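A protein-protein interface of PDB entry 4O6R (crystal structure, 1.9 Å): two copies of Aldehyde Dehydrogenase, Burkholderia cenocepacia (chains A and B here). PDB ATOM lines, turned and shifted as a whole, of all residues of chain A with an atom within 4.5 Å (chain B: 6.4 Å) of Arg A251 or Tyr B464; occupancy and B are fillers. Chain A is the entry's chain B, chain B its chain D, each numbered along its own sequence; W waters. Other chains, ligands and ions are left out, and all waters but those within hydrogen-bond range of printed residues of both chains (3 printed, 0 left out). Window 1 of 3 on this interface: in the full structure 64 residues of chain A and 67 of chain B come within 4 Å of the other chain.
Of the 13 printed residues of chain A, 4 touch a printed residue of chain B.
Printed residues of chain A that touch a printed residue of chain B: Leu A249, Lys A250, Arg A251 and Glu A478.
Among the printed residues, 6 pairs touch across the chains.
Among the printed residues, no Asp or Glu carboxylate lies within 4 Å of a Lys or Arg side-chain nitrogen of the other chain.
Arg A251 touches just one residue of chain B: Tyr B464.
Of chain A, only Leu A249, Lys A250 and Arg A251 come within 4 Å of Tyr B464.
Of the printed residues of chain A, Leu B256 touches Leu A249.
Of the printed residues of chain A, Val B459 touches Glu A478.
Printed residues of chain B within 4 Å of Glu A478: Val B459.
Of the printed residues of chain A, Leu B254 touches Leu A249 (3.9 Å).
The nearest residue of chain B that does not touch Arg A251 is Gly B463 (5.6 Å).
The nearest printed residue of chain A that does not touch Tyr B464 is Val A252 (5.0 Å).
CD1 of Leu A249 touches CD1 of Leu B254, at 3.9 Å.
CG of Leu A249 touches CD1 of Leu B256, at 3.9 Å.
CE2 of Tyr B464 touches O of Leu A249 (3.3 Å).
Lys A250 touches Tyr B464.
Arg A251 touches Tyr B464.
Glu A478 touches Val B459 (OE2 to CG1, 3.6 Å).
Water W2 bridges the backbone carbonyl oxygen of Leu A249 (2.7 Å) and the backbone carbonyl oxygen of Gly B460 (2.8 Å).
Water W1 lies within hydrogen-bond range of the side-chain hydroxyl of Tyr B464 (2.8 Å) and the backbone carbonyl oxygen of Lys A250 (2.8 Å).
Water W3 lies within hydrogen-bond range of a ring nitrogen (NE2) of His A474 (2.8 Å) and the side-chain carboxylate (OD1) of Asp B475 (2.9 Å).
The backbone carbonyl oxygen (O) of Leu B254 is in hydrogen-bond range of the backbone NH (N) of Tyr B464 (2.9 Å).
The backbone carbonyl oxygen of Ser B462 sits at hydrogen-bond distance from the backbone NH of Leu B256 (2.9 Å).
The backbone carbonyl oxygen (O) of Thr A477 is in hydrogen-bond range of the guanidinium group (NH1) of Arg A251.
The guanidinium group (NH2) of Arg A251 is in hydrogen-bond range of the backbone carbonyl oxygen (O) of Asp A475, 3.2 Å away.
O of Gly A227 sits at hydrogen-bond distance from N of Arg A251, 3.0 Å away.
The backbone NH of Ile A229 lies within hydrogen-bond range of the backbone carbonyl oxygen of Arg A251.
Positions printed for both chains: 252, 253 and 475.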
ATOM      1  N   ILE A 147     -26.802  -2.199  -0.777  1.00  0.00           N
ATOM      2  CA  ILE A 147     -26.961  -2.553   0.643  1.00  0.00           C
ATOM      3  C   ILE A 147     -27.856  -1.540   1.343  1.00  0.00           C
ATOM      4  O   ILE A 147     -28.743  -1.934   2.099  1.00  0.00           O
ATOM      5  CB  ILE A 147     -25.594  -2.644   1.363  1.00  0.00           C
ATOM      6  CG1 ILE A 147     -24.767  -3.762   0.721  1.00  0.00           C
ATOM      7  CG2 ILE A 147     -25.769  -2.844   2.867  1.00  0.00           C
ATOM      8  CD1 ILE A 147     -23.315  -3.781   1.142  1.00  0.00           C
ATOM      9  N   GLY A 227     -25.691  -0.169   6.929  1.00  0.00           N
ATOM     10  CA  GLY A 227     -25.697  -1.584   6.512  1.00  0.00           C
ATOM     11  C   GLY A 227     -24.329  -2.219   6.305  1.00  0.00           C
ATOM     12  O   GLY A 227     -24.202  -3.443   6.245  1.00  0.00           O
ATOM     13  N   LYS A 228     -23.323  -1.379   6.127  1.00  0.00           N
ATOM     14  CA  LYS A 228     -21.955  -1.838   5.926  1.00  0.00           C
ATOM     15  C   LYS A 228     -20.982  -0.755   6.367  1.00  0.00           C
ATOM     16  O   LYS A 228     -21.237   0.448   6.175  1.00  0.00           O
ATOM     17  CB  LYS A 228     -21.716  -2.223   4.466  1.00  0.00           C
ATOM     18  CG  LYS A 228     -20.262  -2.611   4.188  1.00  0.00           C
ATOM     19  CD  LYS A 228     -20.019  -3.097   2.770  1.00  0.00           C
ATOM     20  CE  LYS A 228     -18.510  -3.218   2.578  1.00  0.00           C
ATOM     21  NZ  LYS A 228     -18.081  -3.547   1.207  1.00  0.00           N
ATOM     22  N   ILE A 229     -19.887  -1.192   6.982  1.00  0.00           N
ATOM     23  CA  ILE A 229     -18.829  -0.296   7.409  1.00  0.00           C
ATOM     24  C   ILE A 229     -17.548  -0.766   6.704  1.00  0.00           C
ATOM     25  O   ILE A 229     -17.253  -1.964   6.704  1.00  0.00           O
ATOM     26  CB  ILE A 229     -18.647  -0.274   8.948  1.00  0.00           C
ATOM     27  CG1 ILE A 229     -17.557   0.716   9.403  1.00  0.00           C
ATOM     28  CG2 ILE A 229     -18.298  -1.637   9.498  1.00  0.00           C
ATOM     29  CD1 ILE A 229     -17.919   2.168   9.212  1.00  0.00           C
ATOM     30  N   LEU A 249     -25.228  -6.284  13.075  1.00  0.00           N
ATOM     31  CA  LEU A 249     -24.653  -7.267  12.164  1.00  0.00           C
ATOM     32  C   LEU A 249     -24.394  -6.701  10.770  1.00  0.00           C
ATOM     33  O   LEU A 249     -24.480  -7.413   9.766  1.00  0.00           O
ATOM     34  CB  LEU A 249     -25.504  -8.557  12.078  1.00  0.00           C
ATOM     35  CG  LEU A 249     -25.611  -9.450  13.328  1.00  0.00           C
ATOM     36  CD1 LEU A 249     -24.250  -9.742  13.923  1.00  0.00           C
ATOM     37  CD2 LEU A 249     -26.526  -8.876  14.364  1.00  0.00           C
ATOM     38  N   LYS A 250     -24.067  -5.410  10.705  1.00  0.00           N
ATOM     39  CA  LYS A 250     -23.658  -4.809   9.461  1.00  0.00           C
ATOM     40  C   LYS A 250     -22.476  -5.533   8.844  1.00  0.00           C
ATOM     41  O   LYS A 250     -21.641  -6.092   9.535  1.00  0.00           O
ATOM     42  CB  LYS A 250     -23.292  -3.328   9.671  1.00  0.00           C
ATOM     43  CG  LYS A 250     -22.199  -3.034  10.696  1.00  0.00           C
ATOM     44  CD  LYS A 250     -21.712  -1.585  10.592  1.00  0.00           C
ATOM     45  CE  LYS A 250     -22.779  -0.563  10.971  1.00  0.00           C
ATOM     46  NZ  LYS A 250     -23.339  -0.691  12.354  1.00  0.00           N
ATOM     47  N   ARG A 251     -22.415  -5.494   7.508  1.00  0.00           N
ATOM     48  CA  ARG A 251     -21.290  -6.053   6.802  1.00  0.00           C
ATOM     49  C   ARG A 251     -20.048  -5.203   7.073  1.00  0.00           C
ATOM     50  O   ARG A 251     -20.155  -4.019   7.443  1.00  0.00           O
ATOM     51  CB  ARG A 251     -21.594  -6.175   5.326  1.00  0.00           C
ATOM     52  CG  ARG A 251     -22.726  -7.176   5.133  1.00  0.00           C
ATOM     53  CD  ARG A 251     -23.371  -7.143   3.782  1.00  0.00           C
ATOM     54  NE  ARG A 251     -22.384  -7.288   2.723  1.00  0.00           N
ATOM     55  CZ  ARG A 251     -22.705  -7.367   1.433  1.00  0.00           C
ATOM     56  NH1 ARG A 251     -23.974  -7.339   1.068  1.00  0.00           N
ATOM     57  NH2 ARG A 251     -21.753  -7.478   0.511  1.00  0.00           N
ATOM     58  N   VAL A 252     -18.893  -5.835   6.915  1.00  0.00           N
ATOM     59  CA  VAL A 252     -17.629  -5.236   7.285  1.00  0.00           C
ATOM     60  C   VAL A 252     -16.613  -5.478   6.177  1.00  0.00           C
ATOM     61  O   VAL A 252     -16.507  -6.609   5.645  1.00  0.00           O
ATOM     62  CB  VAL A 252     -17.077  -5.848   8.600  1.00  0.00           C
ATOM     63  CG1 VAL A 252     -15.708  -5.272   8.930  1.00  0.00           C
ATOM     64  CG2 VAL A 252     -18.057  -5.601   9.734  1.00  0.00           C
ATOM     65  N   GLN A 253     -15.864  -4.436   5.867  1.00  0.00           N
ATOM     66  CA  GLN A 253     -14.701  -4.520   5.003  1.00  0.00           C
ATOM     67  C   GLN A 253     -13.514  -3.891   5.725  1.00  0.00           C
ATOM     68  O   GLN A 253     -13.624  -2.813   6.313  1.00  0.00           O
ATOM     69  CB  GLN A 253     -15.019  -3.843   3.658  1.00  0.00           C
ATOM     70  CG  GLN A 253     -13.835  -3.598   2.740  1.00  0.00           C
ATOM     71  CD  GLN A 253     -14.245  -3.122   1.355  1.00  0.00           C
ATOM     72  OE1 GLN A 253     -15.440  -2.890   1.067  1.00  0.00           O
ATOM     73  NE2 GLN A 253     -13.269  -2.944   0.500  1.00  0.00           N
ATOM     74  N   HIS A 474     -19.425  -6.306  -6.126  1.00  0.00           N
ATOM     75  CA  HIS A 474     -20.009  -7.429  -5.406  1.00  0.00           C
ATOM     76  C   HIS A 474     -20.109  -7.115  -3.890  1.00  0.00           C
ATOM     77  O   HIS A 474     -21.162  -7.297  -3.284  1.00  0.00           O
ATOM     78  CB  HIS A 474     -19.197  -8.697  -5.680  1.00  0.00           C
ATOM     79  CG  HIS A 474     -19.797  -9.947  -5.119  1.00  0.00           C
ATOM     80  ND1 HIS A 474     -20.635 -10.774  -5.844  1.00  0.00           N
ATOM     81  CD2 HIS A 474     -19.676 -10.517  -3.900  1.00  0.00           C
ATOM     82  CE1 HIS A 474     -20.983 -11.803  -5.101  1.00  0.00           C
ATOM     83  NE2 HIS A 474     -20.435 -11.660  -3.912  1.00  0.00           N
ATOM     84  N   ASP A 475     -19.038  -6.601  -3.306  1.00  0.00           N
ATOM     85  CA  ASP A 475     -19.010  -6.321  -1.868  1.00  0.00           C
ATOM     86  C   ASP A 475     -19.905  -5.123  -1.489  1.00  0.00           C
ATOM     87  O   ASP A 475     -20.113  -4.884  -0.302  1.00  0.00           O
ATOM     88  CB  ASP A 475     -17.589  -5.998  -1.389  1.00  0.00           C
ATOM     89  CG  ASP A 475     -16.637  -7.176  -1.417  1.00  0.00           C
ATOM     90  OD1 ASP A 475     -17.085  -8.314  -1.671  1.00  0.00           O
ATOM     91  OD2 ASP A 475     -15.405  -6.908  -1.163  1.00  0.00           O
ATOM     92  N   THR A 477     -23.021  -4.736  -2.982  1.00  0.00           N
ATOM     93  CA  THR A 477     -24.371  -5.170  -3.294  1.00  0.00           C
ATOM     94  C   THR A 477     -24.705  -6.445  -2.480  1.00  0.00           C
ATOM     95  O   THR A 477     -23.852  -7.002  -1.788  1.00  0.00           O
ATOM     96  CB  THR A 477     -24.540  -5.468  -4.803  1.00  0.00           C
ATOM     97  OG1 THR A 477     -23.501  -6.383  -5.243  1.00  0.00           O
ATOM     98  CG2 THR A 477     -24.461  -4.169  -5.579  1.00  0.00           C
ATOM     99  N   GLU A 478     -25.959  -6.852  -2.573  1.00  0.00           N
ATOM    100  CA  GLU A 478     -26.434  -8.071  -1.945  1.00  0.00           C
ATOM    101  C   GLU A 478     -27.285  -8.809  -2.936  1.00  0.00           C
ATOM    102  O   GLU A 478     -27.986  -8.201  -3.763  1.00  0.00           O
ATOM    103  CB  GLU A 478     -27.250  -7.756  -0.686  1.00  0.00           C
ATOM    104  CG  GLU A 478     -28.486  -6.925  -0.983  1.00  0.00           C
ATOM    105  CD  GLU A 478     -29.128  -6.247   0.213  1.00  0.00           C
ATOM    106  OE1 GLU A 478     -28.437  -6.009   1.239  1.00  0.00           O
ATOM    107  OE2 GLU A 478     -30.343  -5.960   0.126  1.00  0.00           O
ATOM    108  N   VAL B 242     -19.295 -12.949  15.744  1.00  0.00           N
ATOM    109  CA  VAL B 242     -18.612 -11.746  15.257  1.00  0.00           C
ATOM    110  C   VAL B 242     -17.580 -11.323  16.296  1.00  0.00           C
ATOM    111  O   VAL B 242     -16.410 -11.091  15.956  1.00  0.00           O
ATOM    112  CB  VAL B 242     -19.607 -10.632  14.942  1.00  0.00           C
ATOM    113  CG1 VAL B 242     -18.874  -9.314  14.698  1.00  0.00           C
ATOM    114  CG2 VAL B 242     -20.440 -11.029  13.697  1.00  0.00           C
ATOM    115  N   VAL B 252     -16.290 -13.977   8.145  1.00  0.00           N
ATOM    116  CA  VAL B 252     -17.472 -14.419   8.822  1.00  0.00           C
ATOM    117  C   VAL B 252     -18.635 -14.536   7.836  1.00  0.00           C
ATOM    118  O   VAL B 252     -18.832 -13.668   6.991  1.00  0.00           O
ATOM    119  CB  VAL B 252     -17.848 -13.404   9.932  1.00  0.00           C
ATOM    120  CG1 VAL B 252     -19.171 -13.774  10.581  1.00  0.00           C
ATOM    121  CG2 VAL B 252     -16.760 -13.325  10.972  1.00  0.00           C
ATOM    122  N   GLN B 253     -19.395 -15.612   7.956  1.00  0.00           N
ATOM    123  CA  GLN B 253     -20.655 -15.771   7.238  1.00  0.00           C
ATOM    124  C   GLN B 253     -21.734 -16.112   8.267  1.00  0.00           C
ATOM    125  O   GLN B 253     -21.509 -16.942   9.172  1.00  0.00           O
ATOM    126  CB  GLN B 253     -20.528 -16.864   6.188  1.00  0.00           C
ATOM    127  CG  GLN B 253     -21.821 -17.201   5.469  1.00  0.00           C
ATOM    128  CD  GLN B 253     -21.620 -18.195   4.331  1.00  0.00           C
ATOM    129  OE1 GLN B 253     -20.475 -18.456   3.869  1.00  0.00           O
ATOM    130  NE2 GLN B 253     -22.736 -18.737   3.831  1.00  0.00           N
ATOM    131  N   LEU B 254     -22.892 -15.469   8.138  1.00  0.00           N
ATOM    132  CA  LEU B 254     -23.963 -15.582   9.141  1.00  0.00           C
ATOM    133  C   LEU B 254     -25.323 -15.734   8.486  1.00  0.00           C
ATOM    134  O   LEU B 254     -25.698 -14.907   7.650  1.00  0.00           O
ATOM    135  CB  LEU B 254     -24.017 -14.325  10.017  1.00  0.00           C
ATOM    136  CG  LEU B 254     -22.756 -13.832  10.768  1.00  0.00           C
ATOM    137  CD1 LEU B 254     -22.954 -12.446  11.360  1.00  0.00           C
ATOM    138  CD2 LEU B 254     -22.351 -14.816  11.848  1.00  0.00           C
ATOM    139  N   GLU B 255     -26.043 -16.797   8.868  1.00  0.00           N
ATOM    140  CA  GLU B 255     -27.460 -16.957   8.550  1.00  0.00           C
ATOM    141  C   GLU B 255     -28.202 -17.041   9.865  1.00  0.00           C
ATOM    142  O   GLU B 255     -28.092 -18.038  10.584  1.00  0.00           O
ATOM    143  CB  GLU B 255     -27.723 -18.219   7.724  1.00  0.00           C
ATOM    144  CG  GLU B 255     -29.118 -18.272   7.088  1.00  0.00           C
ATOM    145  CD  GLU B 255     -30.178 -19.046   7.869  1.00  0.00           C
ATOM    146  OE1 GLU B 255     -30.598 -20.130   7.393  1.00  0.00           O
ATOM    147  OE2 GLU B 255     -30.636 -18.574   8.935  1.00  0.00           O
ATOM    148  N   LEU B 256     -28.988 -16.014  10.150  1.00  0.00           N
ATOM    149  CA  LEU B 256     -29.529 -15.806  11.479  1.00  0.00           C
ATOM    150  C   LEU B 256     -31.052 -15.895  11.453  1.00  0.00           C
ATOM    151  O   LEU B 256     -31.602 -16.684  10.686  1.00  0.00           O
ATOM    152  CB  LEU B 256     -29.017 -14.470  12.020  1.00  0.00           C
ATOM    153  CG  LEU B 256     -27.491 -14.325  11.896  1.00  0.00           C
ATOM    154  CD1 LEU B 256     -27.050 -12.971  12.410  1.00  0.00           C
ATOM    155  CD2 LEU B 256     -26.765 -15.459  12.626  1.00  0.00           C
ATOM    156  N   GLY B 458     -29.636 -13.850   3.958  1.00  0.00           N
ATOM    157  CA  GLY B 458     -30.436 -12.745   4.482  1.00  0.00           C
ATOM    158  C   GLY B 458     -29.818 -11.384   4.313  1.00  0.00           C
ATOM    159  O   GLY B 458     -28.710 -11.239   3.770  1.00  0.00           O
ATOM    160  N   VAL B 459     -30.563 -10.394   4.769  1.00  0.00           N
ATOM    161  CA  VAL B 459     -30.109  -9.013   4.829  1.00  0.00           C
ATOM    162  C   VAL B 459     -30.287  -8.506   6.259  1.00  0.00           C
ATOM    163  O   VAL B 459     -30.931  -9.161   7.074  1.00  0.00           O
ATOM    164  CB  VAL B 459     -30.851  -8.111   3.831  1.00  0.00           C
ATOM    165  CG1 VAL B 459     -30.681  -8.660   2.415  1.00  0.00           C
ATOM    166  CG2 VAL B 459     -32.328  -7.944   4.207  1.00  0.00           C
ATOM    167  N   GLY B 460     -29.689  -7.358   6.568  1.00  0.00           N
ATOM    168  CA  GLY B 460     -29.811  -6.771   7.927  1.00  0.00           C
ATOM    169  C   GLY B 460     -29.397  -7.756   9.007  1.00  0.00           C
ATOM    170  O   GLY B 460     -28.368  -8.471   8.874  1.00  0.00           O
ATOM    171  N   SER B 462     -30.599 -10.529   9.731  1.00  0.00           N
ATOM    172  CA  SER B 462     -30.646 -11.930   9.298  1.00  0.00           C
ATOM    173  C   SER B 462     -29.280 -12.437   8.776  1.00  0.00           C
ATOM    174  O   SER B 462     -29.123 -13.629   8.454  1.00  0.00           O
ATOM    175  CB  SER B 462     -31.761 -12.129   8.260  1.00  0.00           C
ATOM    176  OG  SER B 462     -33.037 -12.011   8.908  1.00  0.00           O
ATOM    177  N   GLY B 463     -28.292 -11.538   8.733  1.00  0.00           N
ATOM    178  CA  GLY B 463     -26.907 -11.936   8.497  1.00  0.00           C
ATOM    179  C   GLY B 463     -26.386 -11.513   7.138  1.00  0.00           C
ATOM    180  O   GLY B 463     -26.903 -10.572   6.525  1.00  0.00           O
ATOM    181  N   TYR B 464     -25.318 -12.168   6.715  1.00  0.00           N
ATOM    182  CA  TYR B 464     -24.654 -11.852   5.471  1.00  0.00           C
ATOM    183  C   TYR B 464     -23.881 -13.029   4.949  1.00  0.00           C
ATOM    184  O   TYR B 464     -23.532 -13.928   5.698  1.00  0.00           O
ATOM    185  CB  TYR B 464     -23.715 -10.646   5.620  1.00  0.00           C
ATOM    186  CG  TYR B 464     -22.786 -10.572   6.830  1.00  0.00           C
ATOM    187  CD1 TYR B 464     -21.559 -11.238   6.839  1.00  0.00           C
ATOM    188  CD2 TYR B 464     -23.070  -9.732   7.900  1.00  0.00           C
ATOM    189  CE1 TYR B 464     -20.684 -11.114   7.908  1.00  0.00           C
ATOM    190  CE2 TYR B 464     -22.209  -9.601   8.967  1.00  0.00           C
ATOM    191  CZ  TYR B 464     -21.009 -10.288   8.966  1.00  0.00           C
ATOM    192  OH  TYR B 464     -20.132 -10.144  10.021  1.00  0.00           O
ATOM    193  N   GLY B 465     -23.595 -12.989   3.654  1.00  0.00           N
ATOM    194  CA  GLY B 465     -23.058 -14.127   2.955  1.00  0.00           C
ATOM    195  C   GLY B 465     -24.193 -14.940   2.351  1.00  0.00           C
ATOM    196  O   GLY B 465     -25.372 -14.765   2.727  1.00  0.00           O
ATOM    197  N   ARG B 466     -23.840 -15.820   1.414  1.00  0.00           N
ATOM    198  CA  ARG B 466     -24.828 -16.670   0.759  1.00  0.00           C
ATOM    199  C   ARG B 466     -24.353 -18.109   0.693  1.00  0.00           C
ATOM    200  O   ARG B 466     -23.189 -18.377   0.418  1.00  0.00           O
ATOM    201  CB  ARG B 466     -25.139 -16.150  -0.672  1.00  0.00           C
ATOM    202  CG  ARG B 466     -25.842 -14.806  -0.707  1.00  0.00           C
ATOM    203  CD  ARG B 466     -27.285 -14.951  -0.233  1.00  0.00           C
ATOM    204  NE  ARG B 466     -28.047 -13.709  -0.265  1.00  0.00           N
ATOM    205  CZ  ARG B 466     -28.089 -12.793   0.695  1.00  0.00           C
ATOM    206  NH1 ARG B 466     -27.354 -12.897   1.810  1.00  0.00           N
ATOM    207  NH2 ARG B 466     -28.871 -11.733   0.525  1.00  0.00           N
ATOM    208  N   ASP B 475     -17.693 -16.627  -1.786  1.00  0.00           N
ATOM    209  CA  ASP B 475     -17.525 -16.424  -0.355  1.00  0.00           C
ATOM    210  C   ASP B 475     -16.550 -17.421   0.284  1.00  0.00           C
ATOM    211  O   ASP B 475     -16.143 -17.228   1.447  1.00  0.00           O
ATOM    212  CB  ASP B 475     -18.861 -16.595   0.376  1.00  0.00           C
ATOM    213  CG  ASP B 475     -19.802 -15.407   0.229  1.00  0.00           C
ATOM    214  OD1 ASP B 475     -19.437 -14.379  -0.407  1.00  0.00           O
ATOM    215  OD2 ASP B 475     -20.934 -15.546   0.779  1.00  0.00           O
HETATM  216  O   HOH W   1     -20.893  -7.919  11.517  1.00  0.00           O
HETATM  217  O   HOH W   2     -26.133  -7.297   7.645  1.00  0.00           O
HETATM  218  O   HOH W   3     -21.350 -13.976  -2.546  1.00  0.00           O
